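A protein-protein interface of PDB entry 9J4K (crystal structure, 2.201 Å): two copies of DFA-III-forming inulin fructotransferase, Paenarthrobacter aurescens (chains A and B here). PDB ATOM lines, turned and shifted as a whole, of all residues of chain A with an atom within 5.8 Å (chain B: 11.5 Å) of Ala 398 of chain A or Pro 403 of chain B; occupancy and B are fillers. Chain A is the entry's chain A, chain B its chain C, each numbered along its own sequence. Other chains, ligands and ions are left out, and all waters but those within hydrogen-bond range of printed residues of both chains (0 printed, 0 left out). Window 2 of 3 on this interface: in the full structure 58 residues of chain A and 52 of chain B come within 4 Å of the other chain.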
ATOM      1  N   SER A 379       8.254 -18.221 -11.560  1.00  0.00           N
ATOM      2  CA  SER A 379       8.847 -19.540 -11.233  1.00  0.00           C
ATOM      3  C   SER A 379       7.763 -20.626 -11.278  1.00  0.00           C
ATOM      4  O   SER A 379       6.598 -20.327 -11.006  1.00  0.00           O
ATOM      5  CB  SER A 379       9.537 -19.481  -9.903  1.00  0.00           C
ATOM      6  OG  SER A 379      10.411 -18.362  -9.851  1.00  0.00           O
ATOM      7  N   LYS A 380       8.142 -21.852 -11.632  1.00  0.00           N
ATOM      8  CA  LYS A 380       7.253 -23.038 -11.566  1.00  0.00           C
ATOM      9  C   LYS A 380       7.972 -24.151 -10.794  1.00  0.00           C
ATOM     10  O   LYS A 380       9.152 -24.441 -11.105  1.00  0.00           O
ATOM     11  CB  LYS A 380       6.843 -23.455 -12.977  1.00  0.00           C
ATOM     12  CG  LYS A 380       5.760 -22.582 -13.598  1.00  0.00           C
ATOM     13  CD  LYS A 380       6.125 -22.045 -14.952  1.00  0.00           C
ATOM     14  CE  LYS A 380       4.922 -21.610 -15.760  1.00  0.00           C
ATOM     15  NZ  LYS A 380       3.947 -20.855 -14.938  1.00  0.00           N
ATOM     16  N   VAL A 381       7.280 -24.731  -9.814  1.00  0.00           N
ATOM     17  CA  VAL A 381       7.761 -25.895  -9.018  1.00  0.00           C
ATOM     18  C   VAL A 381       6.741 -27.029  -9.175  1.00  0.00           C
ATOM     19  O   VAL A 381       5.592 -26.835  -8.726  1.00  0.00           O
ATOM     20  CB  VAL A 381       7.977 -25.511  -7.542  1.00  0.00           C
ATOM     21  CG1 VAL A 381       8.561 -26.667  -6.744  1.00  0.00           C
ATOM     22  CG2 VAL A 381       8.848 -24.272  -7.406  1.00  0.00           C
ATOM     23  N   LEU A 382       7.142 -28.139  -9.809  1.00  0.00           N
ATOM     24  CA  LEU A 382       6.287 -29.331 -10.080  1.00  0.00           C
ATOM     25  C   LEU A 382       6.922 -30.570  -9.440  1.00  0.00           C
ATOM     26  O   LEU A 382       8.099 -30.858  -9.754  1.00  0.00           O
ATOM     27  CB  LEU A 382       6.151 -29.562 -11.591  1.00  0.00           C
ATOM     28  CG  LEU A 382       5.965 -28.329 -12.467  1.00  0.00           C
ATOM     29  CD1 LEU A 382       5.802 -28.742 -13.924  1.00  0.00           C
ATOM     30  CD2 LEU A 382       4.769 -27.514 -12.011  1.00  0.00           C
ATOM     31  N   ASP A 396       4.565 -14.886  -6.882  1.00  0.00           N
ATOM     32  CA  ASP A 396       4.017 -15.268  -8.213  1.00  0.00           C
ATOM     33  C   ASP A 396       4.479 -16.671  -8.656  1.00  0.00           C
ATOM     34  O   ASP A 396       4.325 -16.977  -9.848  1.00  0.00           O
ATOM     35  CB  ASP A 396       4.362 -14.194  -9.250  1.00  0.00           C
ATOM     36  CG  ASP A 396       5.816 -14.174  -9.689  1.00  0.00           C
ATOM     37  OD1 ASP A 396       6.695 -14.571  -8.883  1.00  0.00           O
ATOM     38  OD2 ASP A 396       6.056 -13.776 -10.844  1.00  0.00           O
ATOM     39  N   THR A 397       4.991 -17.506  -7.750  1.00  0.00           N
ATOM     40  CA  THR A 397       5.445 -18.893  -8.045  1.00  0.00           C
ATOM     41  C   THR A 397       4.224 -19.814  -8.173  1.00  0.00           C
ATOM     42  O   THR A 397       3.487 -19.932  -7.186  1.00  0.00           O
ATOM     43  CB  THR A 397       6.382 -19.416  -6.948  1.00  0.00           C
ATOM     44  OG1 THR A 397       7.492 -18.525  -6.856  1.00  0.00           O
ATOM     45  CG2 THR A 397       6.877 -20.822  -7.206  1.00  0.00           C
ATOM     46  N   ALA A 398       4.037 -20.469  -9.322  1.00  0.00           N
ATOM     47  CA  ALA A 398       3.047 -21.564  -9.488  1.00  0.00           C
ATOM     48  C   ALA A 398       3.631 -22.857  -8.901  1.00  0.00           C
ATOM     49  O   ALA A 398       4.747 -23.245  -9.303  1.00  0.00           O
ATOM     50  CB  ALA A 398       2.659 -21.715 -10.939  1.00  0.00           C
ATOM     51  N   ILE A 399       2.918 -23.489  -7.965  1.00  0.00           N
ATOM     52  CA  ILE A 399       3.403 -24.689  -7.218  1.00  0.00           C
ATOM     53  C   ILE A 399       2.409 -25.839  -7.383  1.00  0.00           C
ATOM     54  O   ILE A 399       1.251 -25.676  -6.971  1.00  0.00           O
ATOM     55  CB  ILE A 399       3.634 -24.376  -5.727  1.00  0.00           C
ATOM     56  CG1 ILE A 399       4.641 -23.242  -5.540  1.00  0.00           C
ATOM     57  CG2 ILE A 399       4.053 -25.640  -4.979  1.00  0.00           C
ATOM     58  CD1 ILE A 399       4.759 -22.743  -4.124  1.00  0.00           C
ATOM     59  N   ARG A 400       2.867 -26.967  -7.931  1.00  0.00           N
ATOM     60  CA  ARG A 400       2.164 -28.270  -7.825  1.00  0.00           C
ATOM     61  C   ARG A 400       2.955 -29.152  -6.868  1.00  0.00           C
ATOM     62  O   ARG A 400       4.066 -29.577  -7.183  1.00  0.00           O
ATOM     63  CB  ARG A 400       1.983 -28.961  -9.178  1.00  0.00           C
ATOM     64  CG  ARG A 400       1.163 -30.240  -9.080  1.00  0.00           C
ATOM     65  CD  ARG A 400       1.664 -31.289 -10.049  1.00  0.00           C
ATOM     66  NE  ARG A 400       1.290 -30.891 -11.385  1.00  0.00           N
ATOM     67  CZ  ARG A 400       2.000 -31.071 -12.490  1.00  0.00           C
ATOM     68  NH1 ARG A 400       3.185 -31.658 -12.470  1.00  0.00           N
ATOM     69  NH2 ARG A 400       1.502 -30.640 -13.632  1.00  0.00           N
ATOM     70  N   ALA B 357       6.324 -34.789 -22.416  1.00  0.00           N
ATOM     71  CA  ALA B 357       6.244 -34.611 -20.944  1.00  0.00           C
ATOM     72  C   ALA B 357       7.392 -33.742 -20.429  1.00  0.00           C
ATOM     73  O   ALA B 357       8.554 -34.030 -20.751  1.00  0.00           O
ATOM     74  CB  ALA B 357       6.209 -35.969 -20.273  1.00  0.00           C
ATOM     75  N   THR B 358       7.074 -32.733 -19.621  1.00  0.00           N
ATOM     76  CA  THR B 358       8.063 -31.976 -18.813  1.00  0.00           C
ATOM     77  C   THR B 358       9.094 -31.327 -19.740  1.00  0.00           C
ATOM     78  O   THR B 358      10.297 -31.555 -19.543  1.00  0.00           O
ATOM     79  CB  THR B 358       8.783 -32.895 -17.811  1.00  0.00           C
ATOM     80  OG1 THR B 358       7.861 -33.882 -17.350  1.00  0.00           O
ATOM     81  CG2 THR B 358       9.374 -32.138 -16.641  1.00  0.00           C
ATOM     82  N   ASN B 359       8.642 -30.547 -20.716  1.00  0.00           N
ATOM     83  CA  ASN B 359       9.536 -29.830 -21.662  1.00  0.00           C
ATOM     84  C   ASN B 359       9.425 -28.330 -21.380  1.00  0.00           C
ATOM     85  O   ASN B 359       8.281 -27.836 -21.244  1.00  0.00           O
ATOM     86  CB  ASN B 359       9.211 -30.183 -23.117  1.00  0.00           C
ATOM     87  CG  ASN B 359       9.467 -31.641 -23.437  1.00  0.00           C
ATOM     88  OD1 ASN B 359      10.616 -32.067 -23.543  1.00  0.00           O
ATOM     89  ND2 ASN B 359       8.401 -32.410 -23.600  1.00  0.00           N
ATOM     90  N   HIS B 360      10.564 -27.639 -21.277  1.00  0.00           N
ATOM     91  CA  HIS B 360      10.626 -26.174 -21.029  1.00  0.00           C
ATOM     92  C   HIS B 360      11.007 -25.454 -22.326  1.00  0.00           C
ATOM     93  O   HIS B 360      12.078 -25.755 -22.868  1.00  0.00           O
ATOM     94  CB  HIS B 360      11.576 -25.845 -19.876  1.00  0.00           C
ATOM     95  CG  HIS B 360      11.616 -24.387 -19.556  1.00  0.00           C
ATOM     96  ND1 HIS B 360      10.464 -23.628 -19.416  1.00  0.00           N
ATOM     97  CD2 HIS B 360      12.654 -23.549 -19.340  1.00  0.00           C
ATOM     98  CE1 HIS B 360      10.793 -22.387 -19.122  1.00  0.00           C
ATOM     99  NE2 HIS B 360      12.135 -22.313 -19.071  1.00  0.00           N
ATOM    100  N   HIS B 369       4.358 -24.629 -28.348  1.00  0.00           N
ATOM    101  CA  HIS B 369       5.314 -25.601 -27.752  1.00  0.00           C
ATOM    102  C   HIS B 369       5.068 -26.958 -28.409  1.00  0.00           C
ATOM    103  O   HIS B 369       6.035 -27.609 -28.801  1.00  0.00           O
ATOM    104  CB  HIS B 369       5.152 -25.677 -26.230  1.00  0.00           C
ATOM    105  CG  HIS B 369       5.502 -24.421 -25.504  1.00  0.00           C
ATOM    106  ND1 HIS B 369       5.730 -24.404 -24.138  1.00  0.00           N
ATOM    107  CD2 HIS B 369       5.659 -23.148 -25.933  1.00  0.00           C
ATOM    108  CE1 HIS B 369       6.007 -23.172 -23.760  1.00  0.00           C
ATOM    109  NE2 HIS B 369       5.966 -22.385 -24.841  1.00  0.00           N
ATOM    110  N   VAL B 381       0.166 -34.840 -23.796  1.00  0.00           N
ATOM    111  CA  VAL B 381       1.013 -33.625 -23.619  1.00  0.00           C
ATOM    112  C   VAL B 381       0.905 -33.184 -22.160  1.00  0.00           C
ATOM    113  O   VAL B 381      -0.198 -32.767 -21.735  1.00  0.00           O
ATOM    114  CB  VAL B 381       0.626 -32.494 -24.589  1.00  0.00           C
ATOM    115  CG1 VAL B 381       1.581 -31.315 -24.460  1.00  0.00           C
ATOM    116  CG2 VAL B 381       0.571 -32.995 -26.022  1.00  0.00           C
ATOM    117  N   LEU B 382       2.015 -33.295 -21.426  1.00  0.00           N
ATOM    118  CA  LEU B 382       2.090 -33.027 -19.968  1.00  0.00           C
ATOM    119  C   LEU B 382       3.164 -31.971 -19.714  1.00  0.00           C
ATOM    120  O   LEU B 382       4.307 -32.177 -20.163  1.00  0.00           O
ATOM    121  CB  LEU B 382       2.442 -34.323 -19.229  1.00  0.00           C
ATOM    122  CG  LEU B 382       1.649 -35.564 -19.623  1.00  0.00           C
ATOM    123  CD1 LEU B 382       2.136 -36.767 -18.830  1.00  0.00           C
ATOM    124  CD2 LEU B 382       0.156 -35.359 -19.421  1.00  0.00           C
ATOM    125  N   ASP B 383       2.805 -30.877 -19.039  1.00  0.00           N
ATOM    126  CA  ASP B 383       3.793 -29.934 -18.457  1.00  0.00           C
ATOM    127  C   ASP B 383       4.809 -29.520 -19.535  1.00  0.00           C
ATOM    128  O   ASP B 383       6.033 -29.441 -19.235  1.00  0.00           O
ATOM    129  CB  ASP B 383       4.428 -30.591 -17.227  1.00  0.00           C
ATOM    130  CG  ASP B 383       3.384 -31.105 -16.245  1.00  0.00           C
ATOM    131  OD1 ASP B 383       2.332 -30.461 -16.128  1.00  0.00           O
ATOM    132  OD2 ASP B 383       3.625 -32.145 -15.597  1.00  0.00           O
ATOM    133  N   SER B 384       4.329 -29.248 -20.752  1.00  0.00           N
ATOM    134  CA  SER B 384       5.172 -28.747 -21.865  1.00  0.00           C
ATOM    135  C   SER B 384       4.665 -27.388 -22.368  1.00  0.00           C
ATOM    136  O   SER B 384       5.048 -26.993 -23.494  1.00  0.00           O
ATOM    137  CB  SER B 384       5.272 -29.797 -22.930  1.00  0.00           C
ATOM    138  OG  SER B 384       5.732 -31.021 -22.357  1.00  0.00           O
ATOM    139  N   GLY B 385       3.897 -26.670 -21.528  1.00  0.00           N
ATOM    140  CA  GLY B 385       3.433 -25.285 -21.769  1.00  0.00           C
ATOM    141  C   GLY B 385       2.039 -25.032 -21.214  1.00  0.00           C
ATOM    142  O   GLY B 385       1.313 -26.009 -20.969  1.00  0.00           O
ATOM    143  N   ALA B 386       1.671 -23.761 -21.022  1.00  0.00           N
ATOM    144  CA  ALA B 386       0.273 -23.315 -20.796  1.00  0.00           C
ATOM    145  C   ALA B 386      -0.603 -23.818 -21.950  1.00  0.00           C
ATOM    146  O   ALA B 386      -0.054 -24.093 -23.040  1.00  0.00           O
ATOM    147  CB  ALA B 386       0.202 -21.808 -20.674  1.00  0.00           C
ATOM    148  N   ALA B 387      -1.913 -23.923 -21.716  1.00  0.00           N
ATOM    149  CA  ALA B 387      -2.923 -24.404 -22.689  1.00  0.00           C
ATOM    150  C   ALA B 387      -2.796 -23.637 -24.012  1.00  0.00           C
ATOM    151  O   ALA B 387      -2.944 -24.256 -25.081  1.00  0.00           O
ATOM    152  CB  ALA B 387      -4.308 -24.262 -22.099  1.00  0.00           C
ATOM    153  N   SER B 388      -2.517 -22.334 -23.947  1.00  0.00           N
ATOM    154  CA  SER B 388      -2.466 -21.426 -25.124  1.00  0.00           C
ATOM    155  C   SER B 388      -1.239 -21.726 -25.999  1.00  0.00           C
ATOM    156  O   SER B 388      -1.129 -21.098 -27.063  1.00  0.00           O
ATOM    157  CB  SER B 388      -2.481 -19.983 -24.687  1.00  0.00           C
ATOM    158  OG  SER B 388      -1.347 -19.698 -23.882  1.00  0.00           O
ATOM    159  N   THR B 389      -0.324 -22.601 -25.559  1.00  0.00           N
ATOM    160  CA  THR B 389       0.906 -22.981 -26.313  1.00  0.00           C
ATOM    161  C   THR B 389       0.805 -24.421 -26.840  1.00  0.00           C
ATOM    162  O   THR B 389       1.700 -24.824 -27.609  1.00  0.00           O
ATOM    163  CB  THR B 389       2.160 -22.780 -25.456  1.00  0.00           C
ATOM    164  OG1 THR B 389       2.204 -23.817 -24.473  1.00  0.00           O
ATOM    165  CG2 THR B 389       2.216 -21.418 -24.793  1.00  0.00           C
ATOM    166  N   ILE B 390      -0.242 -25.169 -26.470  1.00  0.00           N
ATOM    167  CA  ILE B 390      -0.496 -26.563 -26.953  1.00  0.00           C
ATOM    168  C   ILE B 390      -1.670 -26.519 -27.942  1.00  0.00           C
ATOM    169  O   ILE B 390      -2.771 -26.081 -27.540  1.00  0.00           O
ATOM    170  CB  ILE B 390      -0.783 -27.529 -25.784  1.00  0.00           C
ATOM    171  CG1 ILE B 390       0.224 -27.370 -24.641  1.00  0.00           C
ATOM    172  CG2 ILE B 390      -0.855 -28.967 -26.272  1.00  0.00           C
ATOM    173  CD1 ILE B 390       1.663 -27.501 -25.060  1.00  0.00           C
ATOM    174  N   ILE B 399      -4.256 -33.440 -22.515  1.00  0.00           N
ATOM    175  CA  ILE B 399      -3.369 -32.264 -22.277  1.00  0.00           C
ATOM    176  C   ILE B 399      -3.465 -31.861 -20.805  1.00  0.00           C
ATOM    177  O   ILE B 399      -4.563 -31.491 -20.357  1.00  0.00           O
ATOM    178  CB  ILE B 399      -3.744 -31.071 -23.183  1.00  0.00           C
ATOM    179  CG1 ILE B 399      -3.759 -31.442 -24.666  1.00  0.00           C
ATOM    180  CG2 ILE B 399      -2.831 -29.880 -22.913  1.00  0.00           C
ATOM    181  CD1 ILE B 399      -4.365 -30.375 -25.557  1.00  0.00           C
ATOM    182  N   ARG B 400      -2.344 -31.882 -20.095  1.00  0.00           N
ATOM    183  CA  ARG B 400      -2.206 -31.190 -18.795  1.00  0.00           C
ATOM    184  C   ARG B 400      -1.337 -29.958 -19.023  1.00  0.00           C
ATOM    185  O   ARG B 400      -0.143 -30.083 -19.303  1.00  0.00           O
ATOM    186  CB  ARG B 400      -1.614 -32.120 -17.735  1.00  0.00           C
ATOM    187  CG  ARG B 400      -1.522 -31.472 -16.361  1.00  0.00           C
ATOM    188  CD  ARG B 400      -1.172 -32.478 -15.295  1.00  0.00           C
ATOM    189  NE  ARG B 400       0.207 -32.918 -15.431  1.00  0.00           N
ATOM    190  CZ  ARG B 400       0.635 -34.183 -15.388  1.00  0.00           C
ATOM    191  NH1 ARG B 400       1.929 -34.428 -15.513  1.00  0.00           N
ATOM    192  NH2 ARG B 400      -0.210 -35.186 -15.218  1.00  0.00           N
ATOM    193  N   PRO B 401      -1.902 -28.732 -18.913  1.00  0.00           N
ATOM    194  CA  PRO B 401      -1.100 -27.521 -19.035  1.00  0.00           C
ATOM    195  C   PRO B 401      -0.090 -27.462 -17.885  1.00  0.00           C
ATOM    196  O   PRO B 401      -0.375 -27.969 -16.830  1.00  0.00           O
ATOM    197  CB  PRO B 401      -2.094 -26.350 -18.933  1.00  0.00           C
ATOM    198  CG  PRO B 401      -3.471 -26.985 -19.046  1.00  0.00           C
ATOM    199  CD  PRO B 401      -3.315 -28.437 -18.637  1.00  0.00           C
ATOM    200  N   THR B 402       1.069 -26.858 -18.131  1.00  0.00           N
ATOM    201  CA  THR B 402       1.999 -26.384 -17.076  1.00  0.00           C
ATOM    202  C   THR B 402       1.192 -25.530 -16.093  1.00  0.00           C
ATOM    203  O   THR B 402       0.525 -24.588 -16.499  1.00  0.00           O
ATOM    204  CB  THR B 402       3.187 -25.650 -17.706  1.00  0.00           C
ATOM    205  OG1 THR B 402       3.796 -26.549 -18.636  1.00  0.00           O
ATOM    206  CG2 THR B 402       4.200 -25.192 -16.683  1.00  0.00           C
ATOM    207  N   PRO B 403       1.196 -25.852 -14.780  1.00  0.00           N
ATOM    208  CA  PRO B 403       0.398 -25.125 -13.783  1.00  0.00           C
ATOM    209  C   PRO B 403       0.461 -23.591 -13.834  1.00  0.00           C
ATOM    210  O   PRO B 403       1.547 -23.081 -14.089  1.00  0.00           O
ATOM    211  CB  PRO B 403       1.034 -25.612 -12.474  1.00  0.00           C
ATOM    212  CG  PRO B 403       1.397 -27.041 -12.783  1.00  0.00           C
ATOM    213  CD  PRO B 403       1.948 -26.971 -14.189  1.00  0.00           C
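O of Ser 379 of chain A is in hydrogen-bond range of N of Ala 398 of chain A (3.1 Å). The backbone NH (N) of Val 381 of chain A is in hydrogen-bond range of the backbone carbonyl oxygen (O) of Ala 398 of chain A (3.0 Å). O of Asp 383 of chain B lies close to N of Thr 358 of chain B (3.5 Å). OD2 of Asp 383 of chain B lies within salt-bridge range of NH1 of Arg 400 of chain B, at 2.8 Å. The backbone NH (N) of Ser 384 of chain B lies within hydrogen-bond range of the side-chain hydroxyl (OG1) of Thr 402 of chain B (3.5 Å). The backbone NH (N) of Gly 385 of chain B lies within hydrogen-bond range of the side-chain hydroxyl (OG1) of Thr 402 of chain B, at 2.9 Å.
Arg 400 of chain B touches its own counterpart, Arg 400 of chain A.
Among the printed residues, pairs that only touch across the chains: Lys 380 of chain A with Thr 402 of chain B (3.8 Å), Leu 382 of chain A with Pro 403 of chain B (3.5 Å), Ala 398 of chain A with Pro 403 of chain B (3.6 Å) and Arg 400 of chain A with Pro 403 of chain B (3.7 Å).
Lys 380 of chain A touches just these residues of chain B: Thr 402 and Pro 403. Of the printed residues of chain B, Leu 382 of chain A touches Pro 403. No residue of chain B comes within 4 Å of Asp 396 of chain A. No residue of chain B comes within 4 Å of Thr 397 of chain A. Ala 398 of chain A touches one residue of chain B. Of the printed residues of chain A, Asp 383 of chain B touches Arg 400 (2.6 Å). Printed residues of chain A within 4 Å of Arg 400 of chain B: Arg 400 (3.2 Å). Printed residues of chain A within 4 Å of Thr 402 of chain B: Lys 380. Pro 403 of chain B touches just these residues of chain A: Lys 380 (3.4 Å), Leu 382 (3.5 Å), Ala 398 (3.6 Å) and Arg 400 (3.7 Å). The nearest residue of chain B that does not touch Ala 398 of chain A is Thr 402 of chain B (6.6 Å). The nearest residue of chain A that does not touch Pro 403 of chain B is Ile 399 of chain A (5.3 Å). The nearest printed residue of chain A that does not touch Thr 402 of chain B is Leu 382 of chain A (4.8 Å).
Of the 9 printed residues of chain A, 4 touch a printed residue of chain B. Of the 20 printed residues of chain B, 4 touch a printed residue of chain A. Printed residues of chain B that touch a printed residue of chain A: Asp 383, Arg 400, Thr 402 and Pro 403. Among the printed residues, 7 pairs touch across the chains.
NZ of Lys 380 of chain A lies within hydrogen-bond range of O of Pro 403 of chain B. The guanidinium group (NH2) of Arg 400 of chain A is in salt-bridge range of the side-chain carboxylate (OD1) of Asp 383 of chain B. NH2 of Arg 400 of chain A sits close to NE of Arg 400 of chain B (3.2 Å).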
